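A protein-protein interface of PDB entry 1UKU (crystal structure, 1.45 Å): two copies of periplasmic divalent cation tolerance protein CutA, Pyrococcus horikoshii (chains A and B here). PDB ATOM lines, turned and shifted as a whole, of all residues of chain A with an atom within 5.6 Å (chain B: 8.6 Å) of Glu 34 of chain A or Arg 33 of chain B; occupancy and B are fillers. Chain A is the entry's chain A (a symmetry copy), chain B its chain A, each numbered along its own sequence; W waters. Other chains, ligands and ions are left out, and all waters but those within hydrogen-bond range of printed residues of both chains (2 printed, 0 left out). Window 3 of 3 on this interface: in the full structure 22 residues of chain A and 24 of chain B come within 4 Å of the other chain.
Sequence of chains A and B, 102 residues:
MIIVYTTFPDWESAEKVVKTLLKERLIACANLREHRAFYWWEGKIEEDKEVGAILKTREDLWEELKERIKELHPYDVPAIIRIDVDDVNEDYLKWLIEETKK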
ATOM      1  N   TRP A  11      23.685  -2.903 -29.857  1.00  0.00           N
ATOM      2  CA  TRP A  11      23.174  -4.008 -30.595  1.00  0.00           C
ATOM      3  C   TRP A  11      23.204  -3.775 -32.078  1.00  0.00           C
ATOM      4  O   TRP A  11      23.408  -4.735 -32.838  1.00  0.00           O
ATOM      5  CB  TRP A  11      21.721  -4.260 -30.147  1.00  0.00           C
ATOM      6  CG  TRP A  11      21.623  -4.991 -28.858  1.00  0.00           C
ATOM      7  CD1 TRP A  11      21.416  -4.463 -27.633  1.00  0.00           C
ATOM      8  CD2 TRP A  11      21.817  -6.386 -28.677  1.00  0.00           C
ATOM      9  NE1 TRP A  11      21.428  -5.451 -26.686  1.00  0.00           N
ATOM     10  CE2 TRP A  11      21.697  -6.648 -27.311  1.00  0.00           C
ATOM     11  CE3 TRP A  11      22.074  -7.452 -29.553  1.00  0.00           C
ATOM     12  CZ2 TRP A  11      21.817  -7.947 -26.794  1.00  0.00           C
ATOM     13  CZ3 TRP A  11      22.183  -8.718 -29.046  1.00  0.00           C
ATOM     14  CH2 TRP A  11      22.069  -8.959 -27.690  1.00  0.00           C
ATOM     15  N   LEU A  32      25.597 -13.174 -28.744  1.00  0.00           N
ATOM     16  CA  LEU A  32      25.660 -11.769 -28.317  1.00  0.00           C
ATOM     17  C   LEU A  32      24.919 -11.601 -27.020  1.00  0.00           C
ATOM     18  O   LEU A  32      23.802 -12.064 -26.884  1.00  0.00           O
ATOM     19  CB  LEU A  32      25.030 -10.846 -29.348  1.00  0.00           C
ATOM     20  CG  LEU A  32      25.873 -10.542 -30.605  1.00  0.00           C
ATOM     21  CD1 LEU A  32      26.475 -11.751 -31.304  1.00  0.00           C
ATOM     22  CD2 LEU A  32      25.055  -9.688 -31.568  1.00  0.00           C
ATOM     23  N   ARG A  33      25.508 -10.891 -26.077  1.00  0.00           N
ATOM     24  CA  ARG A  33      24.833 -10.578 -24.812  1.00  0.00           C
ATOM     25  C   ARG A  33      25.413  -9.298 -24.214  1.00  0.00           C
ATOM     26  O   ARG A  33      26.581  -9.001 -24.364  1.00  0.00           O
ATOM     27  CB  ARG A  33      24.873 -11.731 -23.799  1.00  0.00           C
ATOM     28  CG  ARG A  33      26.124 -11.832 -22.955  1.00  0.00           C
ATOM     29  CD  ARG A  33      27.297 -12.251 -23.696  1.00  0.00           C
ATOM     30  NE  ARG A  33      28.540 -12.264 -22.886  1.00  0.00           N
ATOM     31  CZ  ARG A  33      29.296 -11.214 -22.584  1.00  0.00           C
ATOM     32  NH1 ARG A  33      28.952 -10.002 -22.932  1.00  0.00           N
ATOM     33  NH2 ARG A  33      30.440 -11.388 -21.930  1.00  0.00           N
ATOM     34  N   GLU A  34      24.554  -8.534 -23.563  1.00  0.00           N
ATOM     35  CA  GLU A  34      24.958  -7.306 -22.890  1.00  0.00           C
ATOM     36  C   GLU A  34      25.941  -7.532 -21.739  1.00  0.00           C
ATOM     37  O   GLU A  34      25.905  -8.550 -21.049  1.00  0.00           O
ATOM     38  CB  GLU A  34      23.696  -6.574 -22.392  1.00  0.00           C
ATOM     39  CG  GLU A  34      22.851  -6.006 -23.520  1.00  0.00           C
ATOM     40  CD  GLU A  34      21.488  -5.500 -23.053  1.00  0.00           C
ATOM     41  OE1 GLU A  34      20.590  -5.308 -23.920  1.00  0.00           O
ATOM     42  OE2 GLU A  34      21.296  -5.284 -21.829  1.00  0.00           O
ATOM     43  N   HIS A  35      26.778  -6.520 -21.521  1.00  0.00           N
ATOM     44  CA  HIS A  35      27.547  -6.442 -20.282  1.00  0.00           C
ATOM     45  C   HIS A  35      27.839  -4.990 -19.982  1.00  0.00           C
ATOM     46  O   HIS A  35      27.596  -4.112 -20.814  1.00  0.00           O
ATOM     47  CB  HIS A  35      28.840  -7.269 -20.340  1.00  0.00           C
ATOM     48  CG  HIS A  35      29.832  -6.774 -21.344  1.00  0.00           C
ATOM     49  ND1 HIS A  35      30.246  -7.523 -22.423  1.00  0.00           N
ATOM     50  CD2 HIS A  35      30.522  -5.609 -21.405  1.00  0.00           C
ATOM     51  CE1 HIS A  35      31.097  -6.805 -23.142  1.00  0.00           C
ATOM     52  NE2 HIS A  35      31.306  -5.652 -22.531  1.00  0.00           N
ATOM     53  N   ARG A  36      28.335  -4.744 -18.786  1.00  0.00           N
ATOM     54  CA  ARG A  36      28.817  -3.428 -18.380  1.00  0.00           C
ATOM     55  C   ARG A  36      30.328  -3.483 -18.296  1.00  0.00           C
ATOM     56  O   ARG A  36      30.928  -4.345 -17.612  1.00  0.00           O
ATOM     57  CB  ARG A  36      28.203  -3.029 -17.040  1.00  0.00           C
ATOM     58  CG  ARG A  36      26.708  -2.748 -17.198  1.00  0.00           C
ATOM     59  CD  ARG A  36      25.982  -2.629 -15.911  1.00  0.00           C
ATOM     60  NE  ARG A  36      24.674  -2.015 -16.106  1.00  0.00           N
ATOM     61  CZ  ARG A  36      23.557  -2.654 -16.421  1.00  0.00           C
ATOM     62  NH1 ARG A  36      23.535  -3.975 -16.599  1.00  0.00           N
ATOM     63  NH2 ARG A  36      22.427  -1.948 -16.556  1.00  0.00           N
ATOM     64  N   LYS A  49      28.017   0.674 -21.214  1.00  0.00           N
ATOM     65  CA  LYS A  49      27.164  -0.475 -21.536  1.00  0.00           C
ATOM     66  C   LYS A  49      27.470  -0.908 -22.952  1.00  0.00           C
ATOM     67  O   LYS A  49      27.550  -0.092 -23.878  1.00  0.00           O
ATOM     68  CB  LYS A  49      25.710  -0.110 -21.442  1.00  0.00           C
ATOM     69  CG  LYS A  49      25.276   0.292 -20.084  1.00  0.00           C
ATOM     70  CD  LYS A  49      23.776   0.460 -20.008  1.00  0.00           C
ATOM     71  CE  LYS A  49      23.019  -0.852 -20.171  1.00  0.00           C
ATOM     72  NZ  LYS A  49      21.520  -0.664 -20.067  1.00  0.00           N
ATOM     73  N   GLU A  50      27.698  -2.199 -23.102  1.00  0.00           N
ATOM     74  CA  GLU A  50      28.149  -2.779 -24.354  1.00  0.00           C
ATOM     75  C   GLU A  50      27.399  -4.064 -24.677  1.00  0.00           C
ATOM     76  O   GLU A  50      26.700  -4.609 -23.853  1.00  0.00           O
ATOM     77  CB  GLU A  50      29.639  -3.114 -24.274  1.00  0.00           C
ATOM     78  CG  GLU A  50      30.593  -1.937 -24.095  1.00  0.00           C
ATOM     79  CD  GLU A  50      32.035  -2.372 -24.290  1.00  0.00           C
ATOM     80  OE1 GLU A  50      32.488  -3.368 -23.710  1.00  0.00           O
ATOM     81  OE2 GLU A  50      32.762  -1.710 -25.060  1.00  0.00           O
ATOM     82  N   VAL A  51      27.638  -4.560 -25.892  1.00  0.00           N
ATOM     83  CA  VAL A  51      27.213  -5.908 -26.278  1.00  0.00           C
ATOM     84  C   VAL A  51      28.464  -6.722 -26.564  1.00  0.00           C
ATOM     85  O   VAL A  51      29.241  -6.355 -27.468  1.00  0.00           O
ATOM     86  CB  VAL A  51      26.254  -5.864 -27.485  1.00  0.00           C
ATOM     87  CG1 VAL A  51      25.889  -7.289 -27.945  1.00  0.00           C
ATOM     88  CG2 VAL A  51      24.996  -5.104 -27.067  1.00  0.00           C
ATOM     89  N   GLY A  52      28.689  -7.773 -25.804  1.00  0.00           N
ATOM     90  CA  GLY A  52      29.795  -8.670 -26.083  1.00  0.00           C
ATOM     91  C   GLY A  52      29.408  -9.716 -27.100  1.00  0.00           C
ATOM     92  O   GLY A  52      28.247 -10.115 -27.132  1.00  0.00           O
ATOM     93  N   TYR B   5      38.430 -14.946 -15.035  1.00  0.00           N
ATOM     94  CA  TYR B   5      36.994 -15.012 -14.753  1.00  0.00           C
ATOM     95  C   TYR B   5      36.799 -15.261 -13.253  1.00  0.00           C
ATOM     96  O   TYR B   5      37.418 -16.133 -12.656  1.00  0.00           O
ATOM     97  CB  TYR B   5      36.340 -16.134 -15.547  1.00  0.00           C
ATOM     98  CG  TYR B   5      34.834 -16.272 -15.432  1.00  0.00           C
ATOM     99  CD1 TYR B   5      34.000 -15.289 -15.908  1.00  0.00           C
ATOM    100  CD2 TYR B   5      34.239 -17.406 -14.846  1.00  0.00           C
ATOM    101  CE1 TYR B   5      32.604 -15.404 -15.825  1.00  0.00           C
ATOM    102  CE2 TYR B   5      32.830 -17.527 -14.759  1.00  0.00           C
ATOM    103  CZ  TYR B   5      32.034 -16.520 -15.264  1.00  0.00           C
ATOM    104  OH  TYR B   5      30.654 -16.633 -15.213  1.00  0.00           O
ATOM    105  N   THR B   6      35.904 -14.500 -12.642  1.00  0.00           N
ATOM    106  CA  THR B   6      35.464 -14.713 -11.276  1.00  0.00           C
ATOM    107  C   THR B   6      33.987 -14.341 -11.197  1.00  0.00           C
ATOM    108  O   THR B   6      33.431 -13.768 -12.121  1.00  0.00           O
ATOM    109  CB  THR B   6      36.354 -13.926 -10.291  1.00  0.00           C
ATOM    110  OG1 THR B   6      36.018 -14.322  -8.948  1.00  0.00           O
ATOM    111  CG2 THR B   6      36.186 -12.432 -10.375  1.00  0.00           C
ATOM    112  N   THR B   7      33.334 -14.726 -10.119  1.00  0.00           N
ATOM    113  CA  THR B   7      31.937 -14.417  -9.941  1.00  0.00           C
ATOM    114  C   THR B   7      31.742 -13.771  -8.612  1.00  0.00           C
ATOM    115  O   THR B   7      32.512 -13.998  -7.687  1.00  0.00           O
ATOM    116  CB  THR B   7      31.030 -15.634 -10.065  1.00  0.00           C
ATOM    117  OG1 THR B   7      31.151 -16.470  -8.893  1.00  0.00           O
ATOM    118  CG2 THR B   7      31.389 -16.491 -11.255  1.00  0.00           C
ATOM    119  N   PHE B   8      30.701 -12.962  -8.535  1.00  0.00           N
ATOM    120  CA  PHE B   8      30.366 -12.164  -7.339  1.00  0.00           C
ATOM    121  C   PHE B   8      28.893 -12.317  -6.993  1.00  0.00           C
ATOM    122  O   PHE B   8      28.080 -12.579  -7.863  1.00  0.00           O
ATOM    123  CB  PHE B   8      30.640 -10.667  -7.572  1.00  0.00           C
ATOM    124  CG  PHE B   8      32.077 -10.324  -7.810  1.00  0.00           C
ATOM    125  CD1 PHE B   8      32.935 -10.147  -6.738  1.00  0.00           C
ATOM    126  CD2 PHE B   8      32.589 -10.184  -9.117  1.00  0.00           C
ATOM    127  CE1 PHE B   8      34.253  -9.823  -6.939  1.00  0.00           C
ATOM    128  CE2 PHE B   8      33.941  -9.848  -9.308  1.00  0.00           C
ATOM    129  CZ  PHE B   8      34.769  -9.691  -8.208  1.00  0.00           C
ATOM    130  N   ASP B  10      26.703  -9.986  -6.052  1.00  0.00           N
ATOM    131  CA  ASP B  10      25.888  -9.019  -6.799  1.00  0.00           C
ATOM    132  C   ASP B  10      26.785  -7.885  -7.277  1.00  0.00           C
ATOM    133  O   ASP B  10      28.028  -7.983  -7.245  1.00  0.00           O
ATOM    134  CB  ASP B  10      24.687  -8.445  -6.009  1.00  0.00           C
ATOM    135  CG  ASP B  10      23.545  -7.908  -6.929  1.00  0.00           C
ATOM    136  OD1 ASP B  10      22.857  -8.727  -7.575  1.00  0.00           O
ATOM    137  OD2 ASP B  10      23.237  -6.681  -7.030  1.00  0.00           O
ATOM    138  N   TRP B  11      26.133  -6.822  -7.735  1.00  0.00           N
ATOM    139  CA  TRP B  11      26.762  -5.767  -8.453  1.00  0.00           C
ATOM    140  C   TRP B  11      27.610  -4.894  -7.572  1.00  0.00           C
ATOM    141  O   TRP B  11      28.645  -4.389  -8.036  1.00  0.00           O
ATOM    142  CB  TRP B  11      25.665  -4.910  -9.116  1.00  0.00           C
ATOM    143  CG  TRP B  11      25.118  -5.515 -10.356  1.00  0.00           C
ATOM    144  CD1 TRP B  11      23.982  -6.233 -10.483  1.00  0.00           C
ATOM    145  CD2 TRP B  11      25.748  -5.518 -11.629  1.00  0.00           C
ATOM    146  NE1 TRP B  11      23.833  -6.656 -11.775  1.00  0.00           N
ATOM    147  CE2 TRP B  11      24.930  -6.242 -12.497  1.00  0.00           C
ATOM    148  CE3 TRP B  11      26.937  -4.959 -12.124  1.00  0.00           C
ATOM    149  CZ2 TRP B  11      25.259  -6.419 -13.849  1.00  0.00           C
ATOM    150  CZ3 TRP B  11      27.252  -5.128 -13.445  1.00  0.00           C
ATOM    151  CH2 TRP B  11      26.433  -5.855 -14.288  1.00  0.00           C
ATOM    152  N   ALA B  14      30.876  -6.695  -6.990  1.00  0.00           N
ATOM    153  CA  ALA B  14      31.581  -6.841  -8.236  1.00  0.00           C
ATOM    154  C   ALA B  14      32.206  -5.493  -8.630  1.00  0.00           C
ATOM    155  O   ALA B  14      33.369  -5.436  -9.020  1.00  0.00           O
ATOM    156  CB  ALA B  14      30.628  -7.318  -9.294  1.00  0.00           C
ATOM    157  N   ALA B  30      37.301  -4.668 -17.254  1.00  0.00           N
ATOM    158  CA  ALA B  30      36.387  -5.686 -16.771  1.00  0.00           C
ATOM    159  C   ALA B  30      35.072  -5.616 -17.558  1.00  0.00           C
ATOM    160  O   ALA B  30      34.643  -4.537 -17.940  1.00  0.00           O
ATOM    161  CB  ALA B  30      36.148  -5.516 -15.333  1.00  0.00           C
ATOM    162  N   ASN B  31      34.484  -6.776 -17.840  1.00  0.00           N
ATOM    163  CA  ASN B  31      33.154  -6.878 -18.416  1.00  0.00           C
ATOM    164  C   ASN B  31      32.298  -7.667 -17.398  1.00  0.00           C
ATOM    165  O   ASN B  31      32.636  -8.795 -17.052  1.00  0.00           O
ATOM    166  CB  ASN B  31      33.176  -7.646 -19.733  1.00  0.00           C
ATOM    167  CG  ASN B  31      33.895  -6.953 -20.874  1.00  0.00           C
ATOM    168  OD1 ASN B  31      34.061  -7.598 -21.913  1.00  0.00           O
ATOM    169  ND2 ASN B  31      34.264  -5.674 -20.749  1.00  0.00           N
ATOM    170  N   LEU B  32      31.220  -7.061 -16.923  1.00  0.00           N
ATOM    171  CA  LEU B  32      30.368  -7.638 -15.877  1.00  0.00           C
ATOM    172  C   LEU B  32      29.006  -7.933 -16.438  1.00  0.00           C
ATOM    173  O   LEU B  32      28.412  -7.093 -17.089  1.00  0.00           O
ATOM    174  CB  LEU B  32      30.204  -6.684 -14.704  1.00  0.00           C
ATOM    175  CG  LEU B  32      31.397  -6.580 -13.730  1.00  0.00           C
ATOM    176  CD1 LEU B  32      32.758  -6.366 -14.373  1.00  0.00           C
ATOM    177  CD2 LEU B  32      31.100  -5.513 -12.680  1.00  0.00           C
ATOM    178  N   ARG B  33      28.472  -9.104 -16.145  1.00  0.00           N
ATOM    179  CA  ARG B  33      27.107  -9.454 -16.555  1.00  0.00           C
ATOM    180  C   ARG B  33      26.532 -10.505 -15.608  1.00  0.00           C
ATOM    181  O   ARG B  33      27.240 -11.344 -15.087  1.00  0.00           O
ATOM    182  CB  ARG B  33      27.008  -9.911 -18.017  1.00  0.00           C
ATOM    183  CG  ARG B  33      27.321 -11.367 -18.281  1.00  0.00           C
ATOM    184  CD  ARG B  33      28.721 -11.703 -18.120  1.00  0.00           C
ATOM    185  NE  ARG B  33      29.011 -13.148 -18.294  1.00  0.00           N
ATOM    186  CZ  ARG B  33      28.837 -14.101 -17.386  1.00  0.00           C
ATOM    187  NH1 ARG B  33      28.297 -13.847 -16.223  1.00  0.00           N
ATOM    188  NH2 ARG B  33      29.233 -15.343 -17.646  1.00  0.00           N
ATOM    189  N   GLU B  34      25.235 -10.412 -15.375  1.00  0.00           N
ATOM    190  CA  GLU B  34      24.524 -11.369 -14.538  1.00  0.00           C
ATOM    191  C   GLU B  34      24.528 -12.794 -15.094  1.00  0.00           C
ATOM    192  O   GLU B  34      24.524 -13.016 -16.305  1.00  0.00           O
ATOM    193  CB  GLU B  34      23.080 -10.870 -14.329  1.00  0.00           C
ATOM    194  CG  GLU B  34      22.997  -9.627 -13.460  1.00  0.00           C
ATOM    195  CD  GLU B  34      21.609  -8.990 -13.452  1.00  0.00           C
ATOM    196  OE1 GLU B  34      21.496  -7.802 -13.040  1.00  0.00           O
ATOM    197  OE2 GLU B  34      20.621  -9.660 -13.849  1.00  0.00           O
ATOM    198  N   HIS B  35      24.474 -13.750 -14.168  1.00  0.00           N
ATOM    199  CA  HIS B  35      24.151 -15.126 -14.534  1.00  0.00           C
ATOM    200  C   HIS B  35      23.503 -15.805 -13.349  1.00  0.00           C
ATOM    201  O   HIS B  35      23.481 -15.258 -12.243  1.00  0.00           O
ATOM    202  CB  HIS B  35      25.380 -15.909 -15.020  1.00  0.00           C
ATOM    203  CG  HIS B  35      26.424 -16.112 -13.969  1.00  0.00           C
ATOM    204  ND1 HIS B  35      27.700 -15.602 -14.068  1.00  0.00           N
ATOM    205  CD2 HIS B  35      26.385 -16.808 -12.805  1.00  0.00           C
ATOM    206  CE1 HIS B  35      28.376 -15.920 -12.973  1.00  0.00           C
ATOM    207  NE2 HIS B  35      27.613 -16.678 -12.204  1.00  0.00           N
ATOM    208  N   ARG B  36      22.958 -16.979 -13.594  1.00  0.00           N
ATOM    209  CA  ARG B  36      22.426 -17.843 -12.544  1.00  0.00           C
ATOM    210  C   ARG B  36      23.361 -19.021 -12.382  1.00  0.00           C
ATOM    211  O   ARG B  36      23.697 -19.746 -13.348  1.00  0.00           O
ATOM    212  CB  ARG B  36      21.014 -18.301 -12.903  1.00  0.00           C
ATOM    213  CG  ARG B  36      20.035 -17.129 -12.832  1.00  0.00           C
ATOM    214  CD  ARG B  36      18.710 -17.418 -13.429  1.00  0.00           C
ATOM    215  NE  ARG B  36      17.724 -16.425 -13.018  1.00  0.00           N
ATOM    216  CZ  ARG B  36      17.494 -15.268 -13.621  1.00  0.00           C
ATOM    217  NH1 ARG B  36      18.180 -14.894 -14.701  1.00  0.00           N
ATOM    218  NH2 ARG B  36      16.544 -14.464 -13.127  1.00  0.00           N
ATOM    219  N   LYS B  49      21.872 -16.208  -7.799  1.00  0.00           N
ATOM    220  CA  LYS B  49      22.042 -15.150  -8.801  1.00  0.00           C
ATOM    221  C   LYS B  49      23.320 -14.404  -8.488  1.00  0.00           C
ATOM    222  O   LYS B  49      23.589 -14.031  -7.341  1.00  0.00           O
ATOM    223  CB  LYS B  49      20.892 -14.183  -8.763  1.00  0.00           C
ATOM    224  CG  LYS B  49      19.583 -14.790  -9.097  1.00  0.00           C
ATOM    225  CD  LYS B  49      18.504 -13.740  -9.231  1.00  0.00           C
ATOM    226  CE  LYS B  49      18.707 -12.826 -10.432  1.00  0.00           C
ATOM    227  NZ  LYS B  49      17.602 -11.798 -10.561  1.00  0.00           N
ATOM    228  N   GLU B  50      24.134 -14.242  -9.515  1.00  0.00           N
ATOM    229  CA  GLU B  50      25.467 -13.682  -9.382  1.00  0.00           C
ATOM    230  C   GLU B  50      25.762 -12.676 -10.484  1.00  0.00           C
ATOM    231  O   GLU B  50      25.041 -12.571 -11.451  1.00  0.00           O
ATOM    232  CB  GLU B  50      26.515 -14.791  -9.465  1.00  0.00           C
ATOM    233  CG  GLU B  50      26.488 -15.841  -8.359  1.00  0.00           C
ATOM    234  CD  GLU B  50      27.724 -16.721  -8.414  1.00  0.00           C
ATOM    235  OE1 GLU B  50      28.092 -17.244  -9.474  1.00  0.00           O
ATOM    236  OE2 GLU B  50      28.378 -16.904  -7.365  1.00  0.00           O
ATOM    237  N   VAL B  51      26.899 -11.995 -10.331  1.00  0.00           N
ATOM    238  CA  VAL B  51      27.470 -11.182 -11.407  1.00  0.00           C
ATOM    239  C   VAL B  51      28.810 -11.791 -11.784  1.00  0.00           C
ATOM    240  O   VAL B  51      29.711 -11.872 -10.925  1.00  0.00           O
ATOM    241  CB  VAL B  51      27.598  -9.706 -10.980  1.00  0.00           C
ATOM    242  CG1 VAL B  51      28.288  -8.875 -12.080  1.00  0.00           C
ATOM    243  CG2 VAL B  51      26.195  -9.165 -10.710  1.00  0.00           C
ATOM    244  N   GLY B  52      28.944 -12.246 -13.012  1.00  0.00           N
ATOM    245  CA  GLY B  52      30.223 -12.736 -13.490  1.00  0.00           C
ATOM    246  C   GLY B  52      31.081 -11.607 -14.010  1.00  0.00           C
ATOM    247  O   GLY B  52      30.538 -10.640 -14.536  1.00  0.00           O
ATOM    248  N   ALA B  53      32.392 -11.741 -13.885  1.00  0.00           N
ATOM    249  CA  ALA B  53      33.357 -10.704 -14.267  1.00  0.00           C
ATOM    250  C   ALA B  53      34.467 -11.313 -15.097  1.00  0.00           C
ATOM    251  O   ALA B  53      35.140 -12.256 -14.670  1.00  0.00           O
ATOM    252  CB  ALA B  53      33.935 -10.047 -13.047  1.00  0.00           C
ATOM    253  N   ILE B  54      34.611 -10.760 -16.284  1.00  0.00           N
ATOM    254  CA  ILE B  54      35.668 -11.095 -17.211  1.00  0.00           C
ATOM    255  C   ILE B  54      36.692  -9.958 -17.126  1.00  0.00           C
ATOM    256  O   ILE B  54      36.424  -8.824 -17.522  1.00  0.00           O
ATOM    257  CB  ILE B  54      35.116 -11.230 -18.648  1.00  0.00           C
ATOM    258  CG1 ILE B  54      34.077 -12.352 -18.745  1.00  0.00           C
ATOM    259  CG2 ILE B  54      36.264 -11.516 -19.624  1.00  0.00           C
ATOM    260  CD1 ILE B  54      33.085 -12.190 -19.905  1.00  0.00           C
HETATM  261  O   HOH W   1      35.066  -4.008 -23.034  1.00  0.00           O
HETATM  262  O   HOH W   2      25.402  -6.160 -17.533  1.00  0.00           O
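A ring nitrogen (NE2) of His 35 of chain A lies close to the side-chain amide oxygen of Asn 31 of chain B, at 3.4 Å.
The backbone carbonyl oxygen (O) of Arg 36 of chain A is in hydrogen-bond range of the backbone NH (N) of Leu 32 of chain B (2.8 Å).
OH of Tyr 5 of chain B sits at hydrogen-bond distance from NH2 of Arg 33 of chain B (3.1 Å).
NE1 of Trp 11 of chain B is in hydrogen-bond range of OE1 of Glu 34 of chain B, 2.9 Å away.
The backbone NH (N) of Gly 52 of chain B sits at hydrogen-bond distance from the backbone carbonyl oxygen (O) of Arg 33 of chain B, 2.8 Å away.
The indole nitrogen (NE1) of Trp 11 of chain A sits at hydrogen-bond distance from the side-chain carboxylate (OE1) of Glu 34 of chain A (2.9 Å).
The guanidinium group (NH1) of Arg 33 of chain A lies within hydrogen-bond range of a ring nitrogen (ND1) of His 35 of chain A, at 2.8 Å.
OE1 of Glu 50 of chain A sits at hydrogen-bond distance from NE2 of His 35 of chain A, at 2.8 Å.
Among the printed residues, merely in contact across the chains: Arg 33 of chain A with Ile 54 of chain B, Glu 34 of chain A with Arg 33 of chain B, His 35 of chain A with Leu 32 of chain B, His 35 of chain A with Arg 33 of chain B, Arg 36 of chain A with Trp 11 of chain B, Arg 36 of chain A with Ala 30 of chain B and Arg 36 of chain A with Asn 31 of chain B.
Printed residues of chain B within 4 Å of Arg 33 of chain A: Ile 54.
Glu 34 of chain A touches just one residue of chain B: Arg 33.
Of the printed residues of chain B, His 35 of chain A touches Asn 31 (3.3 Å), Leu 32 (3.3 Å) and Arg 33 (3.97 Å).
Printed residues of chain B within 4 Å of Arg 36 of chain A: Trp 11, Ala 30, Asn 31 and Leu 32.
Of the printed residues of chain A, Leu 32 of chain B touches His 35 and Arg 36.
Of chain A, only Glu 34 (3.5 Å) and His 35 (3.97 Å) come within 4 Å of Arg 33 of chain B.
The nearest residue of chain A that does not touch Arg 33 of chain B is Arg 33 of chain A (4.2 Å).
The nearest printed residue of chain A that does not touch Trp 11 of chain B is His 35 of chain A (5.9 Å).
Hydrophobic or aromatic side chains of chain A that line the printed part of chain B: His 35.
Along chain A the printed residues that touch a printed residue of chain B span positions 33 to 36.
Among the printed residues, 9 pairs touch across the chains.
Among the printed residues, no Asp or Glu carboxylate lies within 4 Å of a Lys or Arg side-chain nitrogen of the other chain.
Glu 34 of chain A touches Arg 33 of chain B, but with the chains exchanged Arg 33 of chain A does not touch Glu 34 of chain B (6.9 Å).
His 35 of chain A touches Arg 33 of chain B, but with the chains exchanged Arg 33 of chain A does not touch His 35 of chain B (9.0 Å).
Arg 36 of chain A touches Trp 11 of chain B, but with the chains exchanged Trp 11 of chain A does not touch Arg 36 of chain B (14.4 Å).
Arg 36 of chain A touches Leu 32 of chain B, but with the chains exchanged Leu 32 of chain A does not touch Arg 36 of chain B (13.7 Å).
Of the 9 pairs that touch across the chains among the printed residues, none has its exchanged pair printed and touching as well.
Water W1 bridges OE1 of Glu 50 of chain A and ND2 of Asn 31 of chain B.
Water W2 lies within hydrogen-bond range of NH1 of Arg 36 of chain A (3.0 Å) and O of Leu 32 of chain B (3.2 Å).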
